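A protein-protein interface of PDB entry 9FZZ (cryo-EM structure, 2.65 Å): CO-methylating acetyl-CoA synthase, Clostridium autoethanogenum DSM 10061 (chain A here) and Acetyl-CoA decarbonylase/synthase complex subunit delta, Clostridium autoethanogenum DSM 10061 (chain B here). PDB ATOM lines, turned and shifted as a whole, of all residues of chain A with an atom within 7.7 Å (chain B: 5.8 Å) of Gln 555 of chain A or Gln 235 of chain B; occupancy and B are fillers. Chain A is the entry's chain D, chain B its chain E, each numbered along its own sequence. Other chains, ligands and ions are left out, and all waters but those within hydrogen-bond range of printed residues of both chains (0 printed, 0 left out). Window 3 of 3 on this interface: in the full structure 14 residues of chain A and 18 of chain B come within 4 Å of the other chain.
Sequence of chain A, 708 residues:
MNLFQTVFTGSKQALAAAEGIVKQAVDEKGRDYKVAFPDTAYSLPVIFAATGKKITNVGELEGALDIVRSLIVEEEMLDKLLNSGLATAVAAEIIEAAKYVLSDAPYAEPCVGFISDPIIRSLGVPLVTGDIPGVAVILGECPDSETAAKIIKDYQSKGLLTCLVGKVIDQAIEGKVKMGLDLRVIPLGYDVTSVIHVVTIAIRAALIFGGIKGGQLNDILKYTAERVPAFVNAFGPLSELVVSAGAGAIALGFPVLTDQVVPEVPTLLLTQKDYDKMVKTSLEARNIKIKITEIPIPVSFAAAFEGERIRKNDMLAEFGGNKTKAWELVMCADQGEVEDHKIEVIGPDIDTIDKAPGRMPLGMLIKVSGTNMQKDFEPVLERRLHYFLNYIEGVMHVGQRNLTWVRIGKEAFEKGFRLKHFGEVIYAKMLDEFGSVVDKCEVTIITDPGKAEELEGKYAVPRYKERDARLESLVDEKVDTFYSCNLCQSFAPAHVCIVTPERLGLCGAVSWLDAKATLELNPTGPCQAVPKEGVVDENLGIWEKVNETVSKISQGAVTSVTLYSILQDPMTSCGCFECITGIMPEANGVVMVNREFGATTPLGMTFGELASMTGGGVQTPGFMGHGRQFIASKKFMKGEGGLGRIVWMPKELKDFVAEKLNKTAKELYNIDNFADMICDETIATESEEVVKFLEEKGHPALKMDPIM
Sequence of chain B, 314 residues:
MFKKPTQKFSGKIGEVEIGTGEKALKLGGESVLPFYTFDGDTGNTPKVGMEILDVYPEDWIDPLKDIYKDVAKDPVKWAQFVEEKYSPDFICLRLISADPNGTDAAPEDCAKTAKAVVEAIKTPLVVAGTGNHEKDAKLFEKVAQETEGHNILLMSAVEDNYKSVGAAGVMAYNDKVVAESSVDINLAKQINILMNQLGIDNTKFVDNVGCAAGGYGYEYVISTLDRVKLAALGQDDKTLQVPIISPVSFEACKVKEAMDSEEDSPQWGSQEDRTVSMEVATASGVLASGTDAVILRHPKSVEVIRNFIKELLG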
ATOM      1  N   ASN A 486     -24.053  24.797 -19.742  1.00  0.00           N
ATOM      2  CA  ASN A 486     -25.470  24.565 -19.506  1.00  0.00           C
ATOM      3  C   ASN A 486     -26.105  25.724 -18.743  1.00  0.00           C
ATOM      4  O   ASN A 486     -27.052  25.535 -17.980  1.00  0.00           O
ATOM      5  CB  ASN A 486     -25.704  23.245 -18.767  1.00  0.00           C
ATOM      6  CG  ASN A 486     -25.002  23.181 -17.421  1.00  0.00           C
ATOM      7  OD1 ASN A 486     -24.590  24.197 -16.885  1.00  0.00           O
ATOM      8  ND2 ASN A 486     -24.869  21.980 -16.870  1.00  0.00           N
ATOM      9  N   GLN A 489     -29.840  26.241 -19.193  1.00  0.00           N
ATOM     10  CA  GLN A 489     -30.765  25.212 -18.744  1.00  0.00           C
ATOM     11  C   GLN A 489     -31.754  25.726 -17.710  1.00  0.00           C
ATOM     12  O   GLN A 489     -32.699  25.010 -17.372  1.00  0.00           O
ATOM     13  CB  GLN A 489     -30.000  24.017 -18.177  1.00  0.00           C
ATOM     14  CG  GLN A 489     -29.398  23.135 -19.261  1.00  0.00           C
ATOM     15  CD  GLN A 489     -29.025  21.775 -18.727  1.00  0.00           C
ATOM     16  OE1 GLN A 489     -29.104  21.539 -17.533  1.00  0.00           O
ATOM     17  NE2 GLN A 489     -28.625  20.868 -19.609  1.00  0.00           N
ATOM     18  N   PRO A 493     -34.509  23.229 -20.375  1.00  0.00           N
ATOM     19  CA  PRO A 493     -34.018  22.106 -19.551  1.00  0.00           C
ATOM     20  C   PRO A 493     -33.171  21.094 -20.293  1.00  0.00           C
ATOM     21  O   PRO A 493     -32.435  20.345 -19.644  1.00  0.00           O
ATOM     22  CB  PRO A 493     -35.314  21.466 -19.019  1.00  0.00           C
ATOM     23  CG  PRO A 493     -36.338  22.568 -19.062  1.00  0.00           C
ATOM     24  CD  PRO A 493     -35.975  23.386 -20.283  1.00  0.00           C
ATOM     25  N   ALA A 494     -33.254  21.026 -21.615  1.00  0.00           N
ATOM     26  CA  ALA A 494     -32.529  20.028 -22.379  1.00  0.00           C
ATOM     27  C   ALA A 494     -31.342  20.600 -23.142  1.00  0.00           C
ATOM     28  O   ALA A 494     -30.627  19.835 -23.794  1.00  0.00           O
ATOM     29  CB  ALA A 494     -33.475  19.320 -23.356  1.00  0.00           C
ATOM     30  N   VAL A 496     -27.756  21.899 -24.142  1.00  0.00           N
ATOM     31  CA  VAL A 496     -26.335  21.850 -23.831  1.00  0.00           C
ATOM     32  C   VAL A 496     -25.593  22.541 -24.966  1.00  0.00           C
ATOM     33  O   VAL A 496     -25.727  22.144 -26.129  1.00  0.00           O
ATOM     34  CB  VAL A 496     -25.827  20.409 -23.663  1.00  0.00           C
ATOM     35  CG1 VAL A 496     -24.373  20.409 -23.217  1.00  0.00           C
ATOM     36  CG2 VAL A 496     -26.684  19.651 -22.667  1.00  0.00           C
ATOM     37  N   THR A 549     -21.331  13.245 -23.072  1.00  0.00           N
ATOM     38  CA  THR A 549     -21.424  14.452 -22.256  1.00  0.00           C
ATOM     39  C   THR A 549     -22.762  15.153 -22.440  1.00  0.00           C
ATOM     40  O   THR A 549     -23.352  15.634 -21.469  1.00  0.00           O
ATOM     41  CB  THR A 549     -20.277  15.397 -22.588  1.00  0.00           C
ATOM     42  OG1 THR A 549     -19.031  14.689 -22.538  1.00  0.00           O
ATOM     43  CG2 THR A 549     -20.240  16.533 -21.595  1.00  0.00           C
ATOM     44  N   VAL A 550     -23.252  15.231 -23.676  1.00  0.00           N
ATOM     45  CA  VAL A 550     -24.550  15.856 -23.920  1.00  0.00           C
ATOM     46  C   VAL A 550     -25.657  15.053 -23.254  1.00  0.00           C
ATOM     47  O   VAL A 550     -26.595  15.614 -22.680  1.00  0.00           O
ATOM     48  CB  VAL A 550     -24.796  16.026 -25.428  1.00  0.00           C
ATOM     49  CG1 VAL A 550     -26.241  16.435 -25.694  1.00  0.00           C
ATOM     50  CG2 VAL A 550     -23.852  17.074 -25.990  1.00  0.00           C
ATOM     51  N   SER A 551     -25.569  13.727 -23.327  1.00  0.00           N
ATOM     52  CA  SER A 551     -26.573  12.886 -22.685  1.00  0.00           C
ATOM     53  C   SER A 551     -26.569  13.083 -21.177  1.00  0.00           C
ATOM     54  O   SER A 551     -27.630  13.159 -20.553  1.00  0.00           O
ATOM     55  CB  SER A 551     -26.309  11.422 -23.045  1.00  0.00           C
ATOM     56  OG  SER A 551     -27.234  10.555 -22.404  1.00  0.00           O
ATOM     57  N   LYS A 552     -25.387  13.178 -20.574  1.00  0.00           N
ATOM     58  CA  LYS A 552     -25.321  13.335 -19.125  1.00  0.00           C
ATOM     59  C   LYS A 552     -25.797  14.716 -18.686  1.00  0.00           C
ATOM     60  O   LYS A 552     -26.583  14.834 -17.739  1.00  0.00           O
ATOM     61  CB  LYS A 552     -23.900  13.079 -18.632  1.00  0.00           C
ATOM     62  CG  LYS A 552     -23.786  13.116 -17.110  1.00  0.00           C
ATOM     63  CD  LYS A 552     -22.422  12.611 -16.643  1.00  0.00           C
ATOM     64  CE  LYS A 552     -22.354  12.590 -15.109  1.00  0.00           C
ATOM     65  NZ  LYS A 552     -21.022  12.104 -14.615  1.00  0.00           N
ATOM     66  N   ILE A 553     -25.352  15.768 -19.375  1.00  0.00           N
ATOM     67  CA  ILE A 553     -25.679  17.127 -18.946  1.00  0.00           C
ATOM     68  C   ILE A 553     -27.158  17.424 -19.143  1.00  0.00           C
ATOM     69  O   ILE A 553     -27.799  18.032 -18.280  1.00  0.00           O
ATOM     70  CB  ILE A 553     -24.789  18.141 -19.680  1.00  0.00           C
ATOM     71  CG1 ILE A 553     -23.327  17.932 -19.256  1.00  0.00           C
ATOM     72  CG2 ILE A 553     -25.247  19.561 -19.377  1.00  0.00           C
ATOM     73  CD1 ILE A 553     -22.364  18.953 -19.832  1.00  0.00           C
ATOM     74  N   SER A 554     -27.724  17.019 -20.273  1.00  0.00           N
ATOM     75  CA  SER A 554     -29.134  17.269 -20.555  1.00  0.00           C
ATOM     76  C   SER A 554     -30.062  16.331 -19.790  1.00  0.00           C
ATOM     77  O   SER A 554     -31.271  16.333 -20.048  1.00  0.00           O
ATOM     78  CB  SER A 554     -29.409  17.178 -22.064  1.00  0.00           C
ATOM     79  OG  SER A 554     -29.120  15.881 -22.572  1.00  0.00           O
ATOM     80  N   GLN A 555     -29.532  15.555 -18.843  1.00  0.00           N
ATOM     81  CA  GLN A 555     -30.318  14.596 -18.070  1.00  0.00           C
ATOM     82  C   GLN A 555     -31.025  13.603 -18.989  1.00  0.00           C
ATOM     83  O   GLN A 555     -32.177  13.225 -18.762  1.00  0.00           O
ATOM     84  CB  GLN A 555     -31.338  15.306 -17.169  1.00  0.00           C
ATOM     85  CG  GLN A 555     -30.762  16.445 -16.300  1.00  0.00           C
ATOM     86  CD  GLN A 555     -29.755  15.953 -15.271  1.00  0.00           C
ATOM     87  OE1 GLN A 555     -29.650  14.763 -15.018  1.00  0.00           O
ATOM     88  NE2 GLN A 555     -29.002  16.879 -14.677  1.00  0.00           N
ATOM     89  N   GLY A 556     -30.332  13.186 -20.046  1.00  0.00           N
ATOM     90  CA  GLY A 556     -30.846  12.179 -20.946  1.00  0.00           C
ATOM     91  C   GLY A 556     -31.855  12.661 -21.962  1.00  0.00           C
ATOM     92  O   GLY A 556     -32.337  11.849 -22.761  1.00  0.00           O
ATOM     93  N   ALA A 557     -32.181  13.952 -21.975  1.00  0.00           N
ATOM     94  CA  ALA A 557     -33.166  14.460 -22.923  1.00  0.00           C
ATOM     95  C   ALA A 557     -32.649  14.425 -24.355  1.00  0.00           C
ATOM     96  O   ALA A 557     -33.423  14.189 -25.286  1.00  0.00           O
ATOM     97  CB  ALA A 557     -33.579  15.882 -22.544  1.00  0.00           C
ATOM     98  N   VAL A 558     -31.351  14.652 -24.549  1.00  0.00           N
ATOM     99  CA  VAL A 558     -30.715  14.624 -25.860  1.00  0.00           C
ATOM    100  C   VAL A 558     -29.694  13.495 -25.864  1.00  0.00           C
ATOM    101  O   VAL A 558     -28.871  13.396 -24.946  1.00  0.00           O
ATOM    102  CB  VAL A 558     -30.053  15.969 -26.198  1.00  0.00           C
ATOM    103  CG1 VAL A 558     -29.411  15.909 -27.574  1.00  0.00           C
ATOM    104  CG2 VAL A 558     -31.083  17.085 -26.141  1.00  0.00           C
ATOM    105  N   SER B  10     -33.314   3.677 -11.962  1.00  0.00           N
ATOM    106  CA  SER B  10     -32.039   3.180 -11.459  1.00  0.00           C
ATOM    107  C   SER B  10     -31.624   3.888 -10.176  1.00  0.00           C
ATOM    108  O   SER B  10     -30.949   3.285  -9.334  1.00  0.00           O
ATOM    109  CB  SER B  10     -30.950   3.320 -12.528  1.00  0.00           C
ATOM    110  OG  SER B  10     -30.852   4.661 -12.997  1.00  0.00           O
ATOM    111  N   GLY B  11     -32.029   5.150  -9.997  1.00  0.00           N
ATOM    112  CA  GLY B  11     -31.619   5.917  -8.841  1.00  0.00           C
ATOM    113  C   GLY B  11     -32.459   5.650  -7.607  1.00  0.00           C
ATOM    114  O   GLY B  11     -33.513   5.020  -7.648  1.00  0.00           O
ATOM    115  N   ILE B 185     -32.069  23.528 -10.835  1.00  0.00           N
ATOM    116  CA  ILE B 185     -31.472  22.205 -10.667  1.00  0.00           C
ATOM    117  C   ILE B 185     -29.952  22.294 -10.704  1.00  0.00           C
ATOM    118  O   ILE B 185     -29.259  21.583  -9.966  1.00  0.00           O
ATOM    119  CB  ILE B 185     -32.003  21.227 -11.732  1.00  0.00           C
ATOM    120  CG1 ILE B 185     -31.291  19.863 -11.609  1.00  0.00           C
ATOM    121  CG2 ILE B 185     -31.825  21.798 -13.141  1.00  0.00           C
ATOM    122  CD1 ILE B 185     -31.700  18.837 -12.665  1.00  0.00           C
ATOM    123  N   ASN B 186     -29.406  23.154 -11.568  1.00  0.00           N
ATOM    124  CA  ASN B 186     -27.954  23.269 -11.665  1.00  0.00           C
ATOM    125  C   ASN B 186     -27.360  23.857 -10.392  1.00  0.00           C
ATOM    126  O   ASN B 186     -26.280  23.450  -9.959  1.00  0.00           O
ATOM    127  CB  ASN B 186     -27.558  24.091 -12.887  1.00  0.00           C
ATOM    128  CG  ASN B 186     -27.893  23.388 -14.192  1.00  0.00           C
ATOM    129  OD1 ASN B 186     -28.548  23.950 -15.058  1.00  0.00           O
ATOM    130  ND2 ASN B 186     -27.452  22.129 -14.325  1.00  0.00           N
ATOM    131  N   LYS B 189     -27.327  21.147  -7.825  1.00  0.00           N
ATOM    132  CA  LYS B 189     -26.183  20.282  -8.093  1.00  0.00           C
ATOM    133  C   LYS B 189     -24.881  20.929  -7.640  1.00  0.00           C
ATOM    134  O   LYS B 189     -24.019  20.268  -7.056  1.00  0.00           O
ATOM    135  CB  LYS B 189     -26.103  19.947  -9.583  1.00  0.00           C
ATOM    136  CG  LYS B 189     -27.211  19.020 -10.075  1.00  0.00           C
ATOM    137  CD  LYS B 189     -27.204  18.907 -11.611  1.00  0.00           C
ATOM    138  CE  LYS B 189     -25.819  18.514 -12.152  1.00  0.00           C
ATOM    139  NZ  LYS B 189     -25.370  17.213 -11.588  1.00  0.00           N
ATOM    140  N   ARG B 227     -37.693  18.282 -12.006  1.00  0.00           N
ATOM    141  CA  ARG B 227     -36.411  18.031 -12.657  1.00  0.00           C
ATOM    142  C   ARG B 227     -35.421  17.371 -11.708  1.00  0.00           C
ATOM    143  O   ARG B 227     -34.702  16.445 -12.099  1.00  0.00           O
ATOM    144  CB  ARG B 227     -35.849  19.337 -13.211  1.00  0.00           C
ATOM    145  CG  ARG B 227     -36.697  19.909 -14.347  1.00  0.00           C
ATOM    146  CD  ARG B 227     -36.214  21.301 -14.746  1.00  0.00           C
ATOM    147  NE  ARG B 227     -34.877  21.254 -15.326  1.00  0.00           N
ATOM    148  CZ  ARG B 227     -34.195  22.316 -15.730  1.00  0.00           C
ATOM    149  NH1 ARG B 227     -34.694  23.534 -15.638  1.00  0.00           N
ATOM    150  NH2 ARG B 227     -32.974  22.150 -16.240  1.00  0.00           N
ATOM    151  N   LEU B 230     -36.530  13.714 -11.236  1.00  0.00           N
ATOM    152  CA  LEU B 230     -36.276  12.904 -12.423  1.00  0.00           C
ATOM    153  C   LEU B 230     -34.790  12.648 -12.616  1.00  0.00           C
ATOM    154  O   LEU B 230     -34.394  11.550 -13.019  1.00  0.00           O
ATOM    155  CB  LEU B 230     -36.870  13.577 -13.659  1.00  0.00           C
ATOM    156  CG  LEU B 230     -38.403  13.539 -13.746  1.00  0.00           C
ATOM    157  CD1 LEU B 230     -38.853  14.269 -14.994  1.00  0.00           C
ATOM    158  CD2 LEU B 230     -38.932  12.104 -13.751  1.00  0.00           C
ATOM    159  N   ALA B 231     -33.952  13.649 -12.359  1.00  0.00           N
ATOM    160  CA  ALA B 231     -32.513  13.452 -12.505  1.00  0.00           C
ATOM    161  C   ALA B 231     -31.974  12.505 -11.445  1.00  0.00           C
ATOM    162  O   ALA B 231     -31.144  11.642 -11.743  1.00  0.00           O
ATOM    163  CB  ALA B 231     -31.790  14.797 -12.444  1.00  0.00           C
ATOM    164  N   ALA B 232     -32.435  12.643 -10.202  1.00  0.00           N
ATOM    165  CA  ALA B 232     -31.929  11.795  -9.128  1.00  0.00           C
ATOM    166  C   ALA B 232     -32.336  10.341  -9.316  1.00  0.00           C
ATOM    167  O   ALA B 232     -31.536   9.432  -9.075  1.00  0.00           O
ATOM    168  CB  ALA B 232     -32.417  12.314  -7.776  1.00  0.00           C
ATOM    169  N   LEU B 233     -33.572  10.094  -9.744  1.00  0.00           N
ATOM    170  CA  LEU B 233     -34.089   8.733  -9.861  1.00  0.00           C
ATOM    171  C   LEU B 233     -33.891   8.165 -11.263  1.00  0.00           C
ATOM    172  O   LEU B 233     -33.286   7.103 -11.431  1.00  0.00           O
ATOM    173  CB  LEU B 233     -35.577   8.702  -9.486  1.00  0.00           C
ATOM    174  CG  LEU B 233     -35.894   9.005  -8.019  1.00  0.00           C
ATOM    175  CD1 LEU B 233     -37.389   9.058  -7.815  1.00  0.00           C
ATOM    176  CD2 LEU B 233     -35.279   7.962  -7.105  1.00  0.00           C
ATOM    177  N   GLY B 234     -34.427   8.847 -12.272  1.00  0.00           N
ATOM    178  CA  GLY B 234     -34.353   8.325 -13.627  1.00  0.00           C
ATOM    179  C   GLY B 234     -32.941   8.282 -14.178  1.00  0.00           C
ATOM    180  O   GLY B 234     -32.533   7.285 -14.778  1.00  0.00           O
ATOM    181  N   GLN B 235     -32.174   9.350 -13.979  1.00  0.00           N
ATOM    182  CA  GLN B 235     -30.834   9.457 -14.538  1.00  0.00           C
ATOM    183  C   GLN B 235     -29.751   8.987 -13.581  1.00  0.00           C
ATOM    184  O   GLN B 235     -28.574   8.974 -13.955  1.00  0.00           O
ATOM    185  CB  GLN B 235     -30.548  10.907 -14.947  1.00  0.00           C
ATOM    186  CG  GLN B 235     -31.507  11.431 -16.014  1.00  0.00           C
ATOM    187  CD  GLN B 235     -31.488  10.575 -17.279  1.00  0.00           C
ATOM    188  OE1 GLN B 235     -32.536  10.268 -17.839  1.00  0.00           O
ATOM    189  NE2 GLN B 235     -30.289  10.183 -17.727  1.00  0.00           N
ATOM    190  N   ASP B 236     -30.117   8.604 -12.363  1.00  0.00           N
ATOM    191  CA  ASP B 236     -29.162   8.130 -11.377  1.00  0.00           C
ATOM    192  C   ASP B 236     -28.048   9.155 -11.161  1.00  0.00           C
ATOM    193  O   ASP B 236     -26.859   8.834 -11.185  1.00  0.00           O
ATOM    194  CB  ASP B 236     -28.594   6.772 -11.785  1.00  0.00           C
ATOM    195  CG  ASP B 236     -27.874   6.079 -10.648  1.00  0.00           C
ATOM    196  OD1 ASP B 236     -28.549   5.667  -9.683  1.00  0.00           O
ATOM    197  OD2 ASP B 236     -26.636   5.959 -10.704  1.00  0.00           O
ATOM    198  N   ASP B 237     -28.451  10.408 -10.950  1.00  0.00           N
ATOM    199  CA  ASP B 237     -27.510  11.490 -10.679  1.00  0.00           C
ATOM    200  C   ASP B 237     -27.193  11.495  -9.188  1.00  0.00           C
ATOM    201  O   ASP B 237     -28.061  11.809  -8.369  1.00  0.00           O
ATOM    202  CB  ASP B 237     -28.106  12.816 -11.128  1.00  0.00           C
ATOM    203  CG  ASP B 237     -27.120  13.961 -11.040  1.00  0.00           C
ATOM    204  OD1 ASP B 237     -25.924  13.683 -10.831  1.00  0.00           O
ATOM    205  OD2 ASP B 237     -27.534  15.127 -11.172  1.00  0.00           O
ATOM    206  N   LEU B 240     -27.823  14.633  -6.690  1.00  0.00           N
ATOM    207  CA  LEU B 240     -29.168  15.084  -6.361  1.00  0.00           C
ATOM    208  C   LEU B 240     -29.956  14.048  -5.570  1.00  0.00           C
ATOM    209  O   LEU B 240     -31.176  14.183  -5.436  1.00  0.00           O
ATOM    210  CB  LEU B 240     -29.944  15.442  -7.639  1.00  0.00           C
ATOM    211  CG  LEU B 240     -29.468  16.688  -8.395  1.00  0.00           C
ATOM    212  CD1 LEU B 240     -30.198  16.796  -9.723  1.00  0.00           C
ATOM    213  CD2 LEU B 240     -29.685  17.947  -7.560  1.00  0.00           C
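The backbone carbonyl oxygen of Gln 489 of chain A lies within hydrogen-bond range of the guanidinium group of Arg 227 of chain B. The side-chain amide oxygen (OE1) of Gln 235 of chain B sits close to the backbone carbonyl oxygen (O) of Gln 555 of chain A (3.1 Å). OD1 of Asn 186 of chain B lies close to OE1 of Gln 489 of chain A (3.5 Å).
The backbone carbonyl oxygen (O) of Ile 553 of chain A is in hydrogen-bond range of the side-chain amide nitrogen (NE2) of Gln 489 of chain A, 3.2 Å away. The backbone carbonyl oxygen of Ser 551 of chain A sits at hydrogen-bond distance from the backbone NH of Gly 556 of chain A, at 2.7 Å. The backbone NH (N) of Gln 235 of chain B is in hydrogen-bond range of the backbone carbonyl oxygen (O) of Leu 230 of chain B. The backbone carbonyl oxygen of Ala 231 of chain B lies within hydrogen-bond range of the backbone NH of Asp 236 of chain B (3.3 Å). The backbone carbonyl oxygen (O) of Ala 231 of chain B lies within hydrogen-bond range of the backbone NH (N) of Asp 237 of chain B (3.1 Å).
Among the printed residues, pairs that only touch across the chains: Gln 555 of chain A with Ala 231 of chain B (3.3 Å), Pro 493 of chain A with Arg 227 of chain B (3.5 Å), Asn 486 of chain A with Asn 186 of chain B (3.6 Å), Gly 556 of chain A with Gln 235 of chain B (3.8 Å) and Gln 555 of chain A with Ile 185 of chain B (3.9 Å).
Of the printed residues of chain B, Asn 486 of chain A touches Asn 186 (3.6 Å). Lys 552 of chain A touches none of the printed residues of chain B. Gln 555 of chain A touches just these residues of chain B: Ile 185, Ala 231 and Gln 235. Leu 230 of chain B touches none of the printed residues of chain A. Of the printed residues of chain A, Ala 231 of chain B touches Gln 555 (3.3 Å). Gly 234 of chain B touches none of the printed residues of chain A. Gln 235 of chain B touches just these residues of chain A: Gln 555 and Gly 556. The nearest residue of chain B that does not touch Gln 555 of chain A is Lys 189 of chain B (4.1 Å).
Hydrophobic or aromatic side chains of chain B within 4 Å of the printed part of chain A: Ile 185 and Ala 231. Of the 15 printed residues of chain A, 5 touch a printed residue of chain B. Printed residues of chain A that touch a printed residue of chain B: Asn 486, Gln 489, Pro 493, Gln 555 and Gly 556.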
